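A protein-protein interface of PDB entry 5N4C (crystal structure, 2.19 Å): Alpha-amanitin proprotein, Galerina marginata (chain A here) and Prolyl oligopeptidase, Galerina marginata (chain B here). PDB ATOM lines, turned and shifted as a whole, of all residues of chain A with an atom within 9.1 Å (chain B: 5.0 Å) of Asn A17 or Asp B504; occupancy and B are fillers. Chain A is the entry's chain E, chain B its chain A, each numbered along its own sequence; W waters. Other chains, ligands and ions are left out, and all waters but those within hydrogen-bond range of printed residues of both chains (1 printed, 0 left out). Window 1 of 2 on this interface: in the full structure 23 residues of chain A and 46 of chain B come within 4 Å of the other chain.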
ATOM      1  N   ASP A   3     -29.055  -0.095  -4.457  1.00  0.00           N
ATOM      2  CA  ASP A   3     -28.055  -0.949  -3.727  1.00  0.00           C
ATOM      3  C   ASP A   3     -28.288  -2.456  -4.000  1.00  0.00           C
ATOM      4  O   ASP A   3     -27.682  -2.950  -4.948  1.00  0.00           O
ATOM      5  CB  ASP A   3     -27.980  -0.602  -2.227  1.00  0.00           C
ATOM      6  CG  ASP A   3     -26.617  -0.922  -1.594  1.00  0.00           C
ATOM      7  OD1 ASP A   3     -25.996  -1.970  -1.902  1.00  0.00           O
ATOM      8  OD2 ASP A   3     -26.199  -0.138  -0.727  1.00  0.00           O
ATOM      9  N   ALA A   6     -29.285  -2.758  -7.595  1.00  0.00           N
ATOM     10  CA  ALA A   6     -28.186  -2.355  -8.501  1.00  0.00           C
ATOM     11  C   ALA A   6     -27.079  -3.415  -8.707  1.00  0.00           C
ATOM     12  O   ALA A   6     -26.376  -3.365  -9.721  1.00  0.00           O
ATOM     13  CB  ALA A   6     -27.565  -1.032  -8.064  1.00  0.00           C
ATOM     14  N   THR A   7     -26.932  -4.383  -7.787  1.00  0.00           N
ATOM     15  CA  THR A   7     -25.913  -5.473  -7.946  1.00  0.00           C
ATOM     16  C   THR A   7     -26.153  -6.407  -9.154  1.00  0.00           C
ATOM     17  O   THR A   7     -25.285  -7.228  -9.474  1.00  0.00           O
ATOM     18  CB  THR A   7     -25.757  -6.358  -6.676  1.00  0.00           C
ATOM     19  OG1 THR A   7     -26.996  -7.024  -6.378  1.00  0.00           O
ATOM     20  CG2 THR A   7     -25.310  -5.529  -5.460  1.00  0.00           C
ATOM     21  N   LEU A   9     -27.624  -4.950 -12.266  1.00  0.00           N
ATOM     22  CA  LEU A   9     -27.675  -4.153 -13.494  1.00  0.00           C
ATOM     23  C   LEU A   9     -26.653  -4.702 -14.491  1.00  0.00           C
ATOM     24  O   LEU A   9     -25.691  -5.365 -14.083  1.00  0.00           O
ATOM     25  CB  LEU A   9     -27.348  -2.677 -13.223  1.00  0.00           C
ATOM     26  CG  LEU A   9     -28.213  -1.890 -12.240  1.00  0.00           C
ATOM     27  CD1 LEU A   9     -27.725  -0.448 -12.101  1.00  0.00           C
ATOM     28  CD2 LEU A   9     -29.668  -1.915 -12.671  1.00  0.00           C
ATOM     29  N   ILE A  11     -23.855  -3.551 -15.645  1.00  0.00           N
ATOM     30  CA  ILE A  11     -22.895  -2.496 -15.280  1.00  0.00           C
ATOM     31  C   ILE A  11     -21.513  -3.128 -15.016  1.00  0.00           C
ATOM     32  O   ILE A  11     -21.437  -4.303 -14.634  1.00  0.00           O
ATOM     33  CB  ILE A  11     -23.405  -1.704 -14.034  1.00  0.00           C
ATOM     34  CG1 ILE A  11     -22.667  -0.364 -13.898  1.00  0.00           C
ATOM     35  CG2 ILE A  11     -23.308  -2.544 -12.759  1.00  0.00           C
ATOM     36  CD1 ILE A  11     -23.268   0.572 -12.866  1.00  0.00           C
ATOM     37  N   TRP A  12     -20.437  -2.357 -15.204  1.00  0.00           N
ATOM     38  CA  TRP A  12     -19.056  -2.884 -15.149  1.00  0.00           C
ATOM     39  C   TRP A  12     -18.636  -3.570 -13.841  1.00  0.00           C
ATOM     40  O   TRP A  12     -17.934  -4.585 -13.908  1.00  0.00           O
ATOM     41  CB  TRP A  12     -18.016  -1.798 -15.520  1.00  0.00           C
ATOM     42  CG  TRP A  12     -16.614  -2.348 -15.613  1.00  0.00           C
ATOM     43  CD1 TRP A  12     -16.053  -2.981 -16.689  1.00  0.00           C
ATOM     44  CD2 TRP A  12     -15.619  -2.366 -14.572  1.00  0.00           C
ATOM     45  NE1 TRP A  12     -14.777  -3.382 -16.388  1.00  0.00           N
ATOM     46  CE2 TRP A  12     -14.480  -3.020 -15.097  1.00  0.00           C
ATOM     47  CE3 TRP A  12     -15.577  -1.884 -13.248  1.00  0.00           C
ATOM     48  CZ2 TRP A  12     -13.301  -3.209 -14.344  1.00  0.00           C
ATOM     49  CZ3 TRP A  12     -14.416  -2.088 -12.493  1.00  0.00           C
ATOM     50  CH2 TRP A  12     -13.292  -2.740 -13.049  1.00  0.00           C
ATOM     51  N   GLY A  13     -19.020  -3.033 -12.676  1.00  0.00           N
ATOM     52  CA  GLY A  13     -18.541  -3.577 -11.373  1.00  0.00           C
ATOM     53  C   GLY A  13     -19.538  -3.504 -10.243  1.00  0.00           C
ATOM     54  O   GLY A  13     -20.462  -2.695 -10.297  1.00  0.00           O
ATOM     55  N   GLY A  15     -19.819  -2.317  -6.411  1.00  0.00           N
ATOM     56  CA  GLY A  15     -20.715  -1.277  -5.891  1.00  0.00           C
ATOM     57  C   GLY A  15     -20.075   0.097  -5.884  1.00  0.00           C
ATOM     58  O   GLY A  15     -18.957   0.269  -6.358  1.00  0.00           O
ATOM     59  N   CYS A  16     -20.740   1.060  -5.253  1.00  0.00           N
ATOM     60  CA  CYS A  16     -20.429   2.509  -5.375  1.00  0.00           C
ATOM     61  C   CYS A  16     -20.341   3.024  -6.842  1.00  0.00           C
ATOM     62  O   CYS A  16     -19.437   3.781  -7.232  1.00  0.00           O
ATOM     63  CB  CYS A  16     -19.246   2.968  -4.501  1.00  0.00           C
ATOM     64  SG  CYS A  16     -19.781   3.685  -2.919  1.00  0.00           S
ATOM     65  N   ASN A  17     -21.328   2.582  -7.621  1.00  0.00           N
ATOM     66  CA  ASN A  17     -21.594   3.071  -8.991  1.00  0.00           C
ATOM     67  C   ASN A  17     -20.372   3.090  -9.933  1.00  0.00           C
ATOM     68  O   ASN A  17     -19.946   4.160 -10.401  1.00  0.00           O
ATOM     69  CB  ASN A  17     -22.265   4.476  -8.912  1.00  0.00           C
ATOM     70  CG  ASN A  17     -22.769   4.977 -10.243  1.00  0.00           C
ATOM     71  OD1 ASN A  17     -23.000   4.188 -11.151  1.00  0.00           O
ATOM     72  ND2 ASN A  17     -22.951   6.291 -10.364  1.00  0.00           N
ATOM     73  N   PRO A  18     -19.801   1.901 -10.226  1.00  0.00           N
ATOM     74  CA  PRO A  18     -18.652   1.870 -11.161  1.00  0.00           C
ATOM     75  C   PRO A  18     -19.119   1.631 -12.610  1.00  0.00           C
ATOM     76  O   PRO A  18     -19.124   0.491 -13.096  1.00  0.00           O
ATOM     77  CB  PRO A  18     -17.777   0.734 -10.608  1.00  0.00           C
ATOM     78  CG  PRO A  18     -18.684  -0.081  -9.741  1.00  0.00           C
ATOM     79  CD  PRO A  18     -20.061   0.543  -9.698  1.00  0.00           C
ATOM     80  N   TRP A  19     -19.476   2.731 -13.281  1.00  0.00           N
ATOM     81  CA  TRP A  19     -20.129   2.697 -14.602  1.00  0.00           C
ATOM     82  C   TRP A  19     -19.168   2.627 -15.809  1.00  0.00           C
ATOM     83  O   TRP A  19     -19.630   2.610 -16.960  1.00  0.00           O
ATOM     84  CB  TRP A  19     -21.137   3.863 -14.750  1.00  0.00           C
ATOM     85  CG  TRP A  19     -20.587   5.292 -14.554  1.00  0.00           C
ATOM     86  CD1 TRP A  19     -20.478   5.990 -13.373  1.00  0.00           C
ATOM     87  CD2 TRP A  19     -20.104   6.170 -15.578  1.00  0.00           C
ATOM     88  NE1 TRP A  19     -19.935   7.239 -13.604  1.00  0.00           N
ATOM     89  CE2 TRP A  19     -19.701   7.377 -14.946  1.00  0.00           C
ATOM     90  CE3 TRP A  19     -19.974   6.058 -16.974  1.00  0.00           C
ATOM     91  CZ2 TRP A  19     -19.187   8.466 -15.665  1.00  0.00           C
ATOM     92  CZ3 TRP A  19     -19.449   7.134 -17.689  1.00  0.00           C
ATOM     93  CH2 TRP A  19     -19.064   8.326 -17.028  1.00  0.00           C
ATOM     94  N   THR A  20     -17.842   2.590 -15.549  1.00  0.00           N
ATOM     95  CA  THR A  20     -16.781   2.407 -16.576  1.00  0.00           C
ATOM     96  C   THR A  20     -15.645   1.501 -16.106  1.00  0.00           C
ATOM     97  O   THR A  20     -15.532   1.190 -14.916  1.00  0.00           O
ATOM     98  CB  THR A  20     -16.222   3.787 -17.070  1.00  0.00           C
ATOM     99  OG1 THR A  20     -16.696   3.972 -18.405  1.00  0.00           O
ATOM    100  CG2 THR A  20     -14.775   4.044 -16.949  1.00  0.00           C
ATOM    101  N   ALA A  21     -14.790   1.106 -17.055  1.00  0.00           N
ATOM    102  CA  ALA A  21     -13.557   0.347 -16.743  1.00  0.00           C
ATOM    103  C   ALA A  21     -12.535   1.141 -15.897  1.00  0.00           C
ATOM    104  O   ALA A  21     -11.865   0.567 -15.042  1.00  0.00           O
ATOM    105  CB  ALA A  21     -12.909  -0.156 -18.028  1.00  0.00           C
ATOM    106  N   GLU A  22     -12.407   2.443 -16.158  1.00  0.00           N
ATOM    107  CA  GLU A  22     -11.536   3.351 -15.365  1.00  0.00           C
ATOM    108  C   GLU A  22     -11.959   3.660 -13.906  1.00  0.00           C
ATOM    109  O   GLU A  22     -11.197   4.286 -13.159  1.00  0.00           O
ATOM    110  CB  GLU A  22     -11.265   4.656 -16.143  1.00  0.00           C
ATOM    111  CG  GLU A  22     -10.152   4.542 -17.183  1.00  0.00           C
ATOM    112  CD  GLU A  22     -10.477   3.640 -18.353  1.00  0.00           C
ATOM    113  OE1 GLU A  22     -11.636   3.677 -18.813  1.00  0.00           O
ATOM    114  OE2 GLU A  22      -9.570   2.909 -18.820  1.00  0.00           O
ATOM    115  N   HIS A  23     -13.134   3.190 -13.498  1.00  0.00           N
ATOM    116  CA  HIS A  23     -13.514   3.157 -12.071  1.00  0.00           C
ATOM    117  C   HIS A  23     -12.732   2.100 -11.252  1.00  0.00           C
ATOM    118  O   HIS A  23     -12.940   2.030 -10.031  1.00  0.00           O
ATOM    119  CB  HIS A  23     -15.037   2.922 -11.908  1.00  0.00           C
ATOM    120  CG  HIS A  23     -15.870   4.133 -12.209  1.00  0.00           C
ATOM    121  ND1 HIS A  23     -16.100   4.588 -13.491  1.00  0.00           N
ATOM    122  CD2 HIS A  23     -16.528   4.988 -11.384  1.00  0.00           C
ATOM    123  CE1 HIS A  23     -16.859   5.668 -13.445  1.00  0.00           C
ATOM    124  NE2 HIS A  23     -17.141   5.926 -12.181  1.00  0.00           N
ATOM    125  N   VAL A  24     -11.869   1.293 -11.897  1.00  0.00           N
ATOM    126  CA  VAL A  24     -11.041   0.258 -11.210  1.00  0.00           C
ATOM    127  C   VAL A  24     -10.660   0.557  -9.740  1.00  0.00           C
ATOM    128  O   VAL A  24     -10.780  -0.347  -8.897  1.00  0.00           O
ATOM    129  CB  VAL A  24      -9.731  -0.140 -11.998  1.00  0.00           C
ATOM    130  CG1 VAL A  24     -10.016  -1.093 -13.146  1.00  0.00           C
ATOM    131  CG2 VAL A  24      -8.949   1.087 -12.451  1.00  0.00           C
ATOM    132  N   GLN A  26     -11.440   1.444  -6.319  1.00  0.00           N
ATOM    133  CA  GLN A  26     -12.563   1.513  -5.372  1.00  0.00           C
ATOM    134  C   GLN A  26     -12.096   1.590  -3.926  1.00  0.00           C
ATOM    135  O   GLN A  26     -12.930   1.515  -3.018  1.00  0.00           O
ATOM    136  CB  GLN A  26     -13.396   0.225  -5.495  1.00  0.00           C
ATOM    137  CG  GLN A  26     -14.105   0.013  -6.828  1.00  0.00           C
ATOM    138  CD  GLN A  26     -15.252   0.978  -7.033  1.00  0.00           C
ATOM    139  OE1 GLN A  26     -15.180   1.855  -7.892  1.00  0.00           O
ATOM    140  NE2 GLN A  26     -16.315   0.827  -6.241  1.00  0.00           N
ATOM    141  N   ALA A  29     -13.788   4.567  -1.241  1.00  0.00           N
ATOM    142  CA  ALA A  29     -15.126   4.380  -0.623  1.00  0.00           C
ATOM    143  C   ALA A  29     -15.321   3.028   0.086  1.00  0.00           C
ATOM    144  O   ALA A  29     -16.329   2.833   0.773  1.00  0.00           O
ATOM    145  CB  ALA A  29     -16.215   4.578  -1.668  1.00  0.00           C
ATOM    146  N   LYS B 377     -27.650  16.363  -5.139  1.00  0.00           N
ATOM    147  CA  LYS B 377     -26.963  16.398  -6.417  1.00  0.00           C
ATOM    148  C   LYS B 377     -27.669  17.424  -7.312  1.00  0.00           C
ATOM    149  O   LYS B 377     -28.753  17.135  -7.853  1.00  0.00           O
ATOM    150  CB  LYS B 377     -26.987  14.997  -7.045  1.00  0.00           C
ATOM    151  CG  LYS B 377     -26.250  14.857  -8.367  1.00  0.00           C
ATOM    152  CD  LYS B 377     -26.201  13.399  -8.811  1.00  0.00           C
ATOM    153  CE  LYS B 377     -25.148  12.617  -8.005  1.00  0.00           C
ATOM    154  NZ  LYS B 377     -25.510  11.199  -7.951  1.00  0.00           N
ATOM    155  N   VAL B 380     -25.659  17.764 -11.516  1.00  0.00           N
ATOM    156  CA  VAL B 380     -24.731  16.630 -11.489  1.00  0.00           C
ATOM    157  C   VAL B 380     -23.505  16.853 -10.585  1.00  0.00           C
ATOM    158  O   VAL B 380     -22.484  16.164 -10.732  1.00  0.00           O
ATOM    159  CB  VAL B 380     -24.312  16.193 -12.918  1.00  0.00           C
ATOM    160  CG1 VAL B 380     -23.970  14.695 -12.946  1.00  0.00           C
ATOM    161  CG2 VAL B 380     -25.401  16.469 -13.944  1.00  0.00           C
ATOM    162  N   ALA B 404     -18.152  14.357  -6.634  1.00  0.00           N
ATOM    163  CA  ALA B 404     -19.040  13.365  -6.040  1.00  0.00           C
ATOM    164  C   ALA B 404     -18.638  13.119  -4.587  1.00  0.00           C
ATOM    165  O   ALA B 404     -17.431  13.098  -4.268  1.00  0.00           O
ATOM    166  CB  ALA B 404     -18.963  12.073  -6.822  1.00  0.00           C
ATOM    167  N   PHE B 423     -12.940  14.987 -11.042  1.00  0.00           N
ATOM    168  CA  PHE B 423     -12.077  14.850 -12.200  1.00  0.00           C
ATOM    169  C   PHE B 423     -10.624  15.216 -11.888  1.00  0.00           C
ATOM    170  O   PHE B 423      -9.721  14.619 -12.465  1.00  0.00           O
ATOM    171  CB  PHE B 423     -12.602  15.650 -13.387  1.00  0.00           C
ATOM    172  CG  PHE B 423     -13.919  15.139 -13.934  1.00  0.00           C
ATOM    173  CD1 PHE B 423     -14.026  13.844 -14.431  1.00  0.00           C
ATOM    174  CD2 PHE B 423     -15.050  15.958 -13.945  1.00  0.00           C
ATOM    175  CE1 PHE B 423     -15.227  13.371 -14.937  1.00  0.00           C
ATOM    176  CE2 PHE B 423     -16.253  15.486 -14.454  1.00  0.00           C
ATOM    177  CZ  PHE B 423     -16.337  14.186 -14.962  1.00  0.00           C
ATOM    178  N   THR B 501     -28.885   5.407 -13.360  1.00  0.00           N
ATOM    179  CA  THR B 501     -27.520   5.534 -12.872  1.00  0.00           C
ATOM    180  C   THR B 501     -27.001   6.894 -13.357  1.00  0.00           C
ATOM    181  O   THR B 501     -27.131   7.222 -14.534  1.00  0.00           O
ATOM    182  CB  THR B 501     -26.612   4.398 -13.419  1.00  0.00           C
ATOM    183  OG1 THR B 501     -26.841   4.262 -14.798  1.00  0.00           O
ATOM    184  CG2 THR B 501     -26.898   3.085 -12.676  1.00  0.00           C
ATOM    185  N   SER B 502     -26.419   7.679 -12.463  1.00  0.00           N
ATOM    186  CA  SER B 502     -25.833   8.978 -12.843  1.00  0.00           C
ATOM    187  C   SER B 502     -24.394   8.846 -13.275  1.00  0.00           C
ATOM    188  O   SER B 502     -23.588   8.207 -12.596  1.00  0.00           O
ATOM    189  CB  SER B 502     -25.878   9.955 -11.669  1.00  0.00           C
ATOM    190  OG  SER B 502     -27.221  10.314 -11.429  1.00  0.00           O
ATOM    191  N   ALA B 503     -24.058   9.471 -14.390  1.00  0.00           N
ATOM    192  CA  ALA B 503     -22.665   9.522 -14.868  1.00  0.00           C
ATOM    193  C   ALA B 503     -21.895  10.595 -14.116  1.00  0.00           C
ATOM    194  O   ALA B 503     -21.611  11.661 -14.661  1.00  0.00           O
ATOM    195  CB  ALA B 503     -22.620   9.757 -16.378  1.00  0.00           C
ATOM    196  N   ASP B 504     -21.557  10.290 -12.871  1.00  0.00           N
ATOM    197  CA  ASP B 504     -20.949  11.259 -11.963  1.00  0.00           C
ATOM    198  C   ASP B 504     -19.478  11.526 -12.267  1.00  0.00           C
ATOM    199  O   ASP B 504     -18.823  10.682 -12.870  1.00  0.00           O
ATOM    200  CB  ASP B 504     -21.017  10.766 -10.512  1.00  0.00           C
ATOM    201  CG  ASP B 504     -22.428  10.717  -9.968  1.00  0.00           C
ATOM    202  OD1 ASP B 504     -23.211  11.607 -10.321  1.00  0.00           O
ATOM    203  OD2 ASP B 504     -22.754   9.805  -9.171  1.00  0.00           O
ATOM    204  N   PRO B 505     -18.955  12.682 -11.812  1.00  0.00           N
ATOM    205  CA  PRO B 505     -17.511  12.888 -11.800  1.00  0.00           C
ATOM    206  C   PRO B 505     -16.772  11.787 -11.006  1.00  0.00           C
ATOM    207  O   PRO B 505     -17.325  11.190 -10.063  1.00  0.00           O
ATOM    208  CB  PRO B 505     -17.337  14.247 -11.094  1.00  0.00           C
ATOM    209  CG  PRO B 505     -18.665  14.938 -11.259  1.00  0.00           C
ATOM    210  CD  PRO B 505     -19.678  13.828 -11.230  1.00  0.00           C
ATOM    211  N   PHE B 506     -15.533  11.529 -11.414  1.00  0.00           N
ATOM    212  CA  PHE B 506     -14.702  10.517 -10.771  1.00  0.00           C
ATOM    213  C   PHE B 506     -13.256  10.816 -11.129  1.00  0.00           C
ATOM    214  O   PHE B 506     -13.005  11.475 -12.134  1.00  0.00           O
ATOM    215  CB  PHE B 506     -15.132   9.091 -11.229  1.00  0.00           C
ATOM    216  CG  PHE B 506     -14.905   8.817 -12.704  1.00  0.00           C
ATOM    217  CD1 PHE B 506     -15.829   9.223 -13.650  1.00  0.00           C
ATOM    218  CD2 PHE B 506     -13.779   8.116 -13.139  1.00  0.00           C
ATOM    219  CE1 PHE B 506     -15.621   8.988 -15.002  1.00  0.00           C
ATOM    220  CE2 PHE B 506     -13.576   7.850 -14.485  1.00  0.00           C
ATOM    221  CZ  PHE B 506     -14.498   8.309 -15.422  1.00  0.00           C
HETATM  222  O   HOH W   1     -26.282   6.752  -9.859  1.00  0.00           O
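Of the 19 printed residues of chain A, 4 touch a printed residue of chain B.
Among the printed residues, 8 pairs touch across the chains.
Asn A17 touches just these residues of chain B: Ser B502 (3.0 Å) and Asp B504 (3.7 Å).
Of chain A, only Asn A17 (3.7 Å) and Trp A19 (3.5 Å) come within 4 Å of Asp B504.
Of chain A, only Trp A19 comes within 4 Å of Ala B503.
No residue of chain A comes within 4 Å of Pro B505.
Of the printed residues of chain B, Leu A9 touches Thr B501.
Of the printed residues of chain A, Thr B501 touches Leu A9.
The nearest residue of chain A that does not touch Asp B504 is His A23 (5.1 Å).
The nearest printed residue of chain A that does not touch Phe B506 is Glu A22 (4.3 Å).
Water W1 lies within hydrogen-bond range of the backbone NH (N) of Ser B502 and the side-chain amide nitrogen (ND2) of Asn A17.
Among the printed residues, pairs that only touch across the chains: Trp A19 with Asp B504 (3.5 Å), Trp A19 with Ala B503 (3.7 Å), Trp A19 with Phe B506 (3.7 Å), Leu A9 with Thr B501 (3.7 Å), His A23 with Phe B506 (3.7 Å), Asn A17 with Asp B504 (3.7 Å) and Trp A19 with Ser B502 (3.9 Å).
The side-chain amino group (NZ) of Lys B377 is in salt-bridge range of the side-chain carboxylate (OD2) of Asp B504 (3.3 Å).
A ring nitrogen (NE2) of His A23 sits at hydrogen-bond distance from the indole nitrogen of Trp A19 (3.4 Å).
The backbone carbonyl oxygen of His A23 sits close to the side-chain amide oxygen of Gln A26 (3.1 Å).
A ring nitrogen (ND1) of His A23 is in hydrogen-bond range of the backbone NH (N) of Thr A20 (3.4 Å).
The backbone carbonyl oxygen (O) of Ser B502 sits at hydrogen-bond distance from the side-chain amide nitrogen (ND2) of Asn A17 (3.0 Å).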
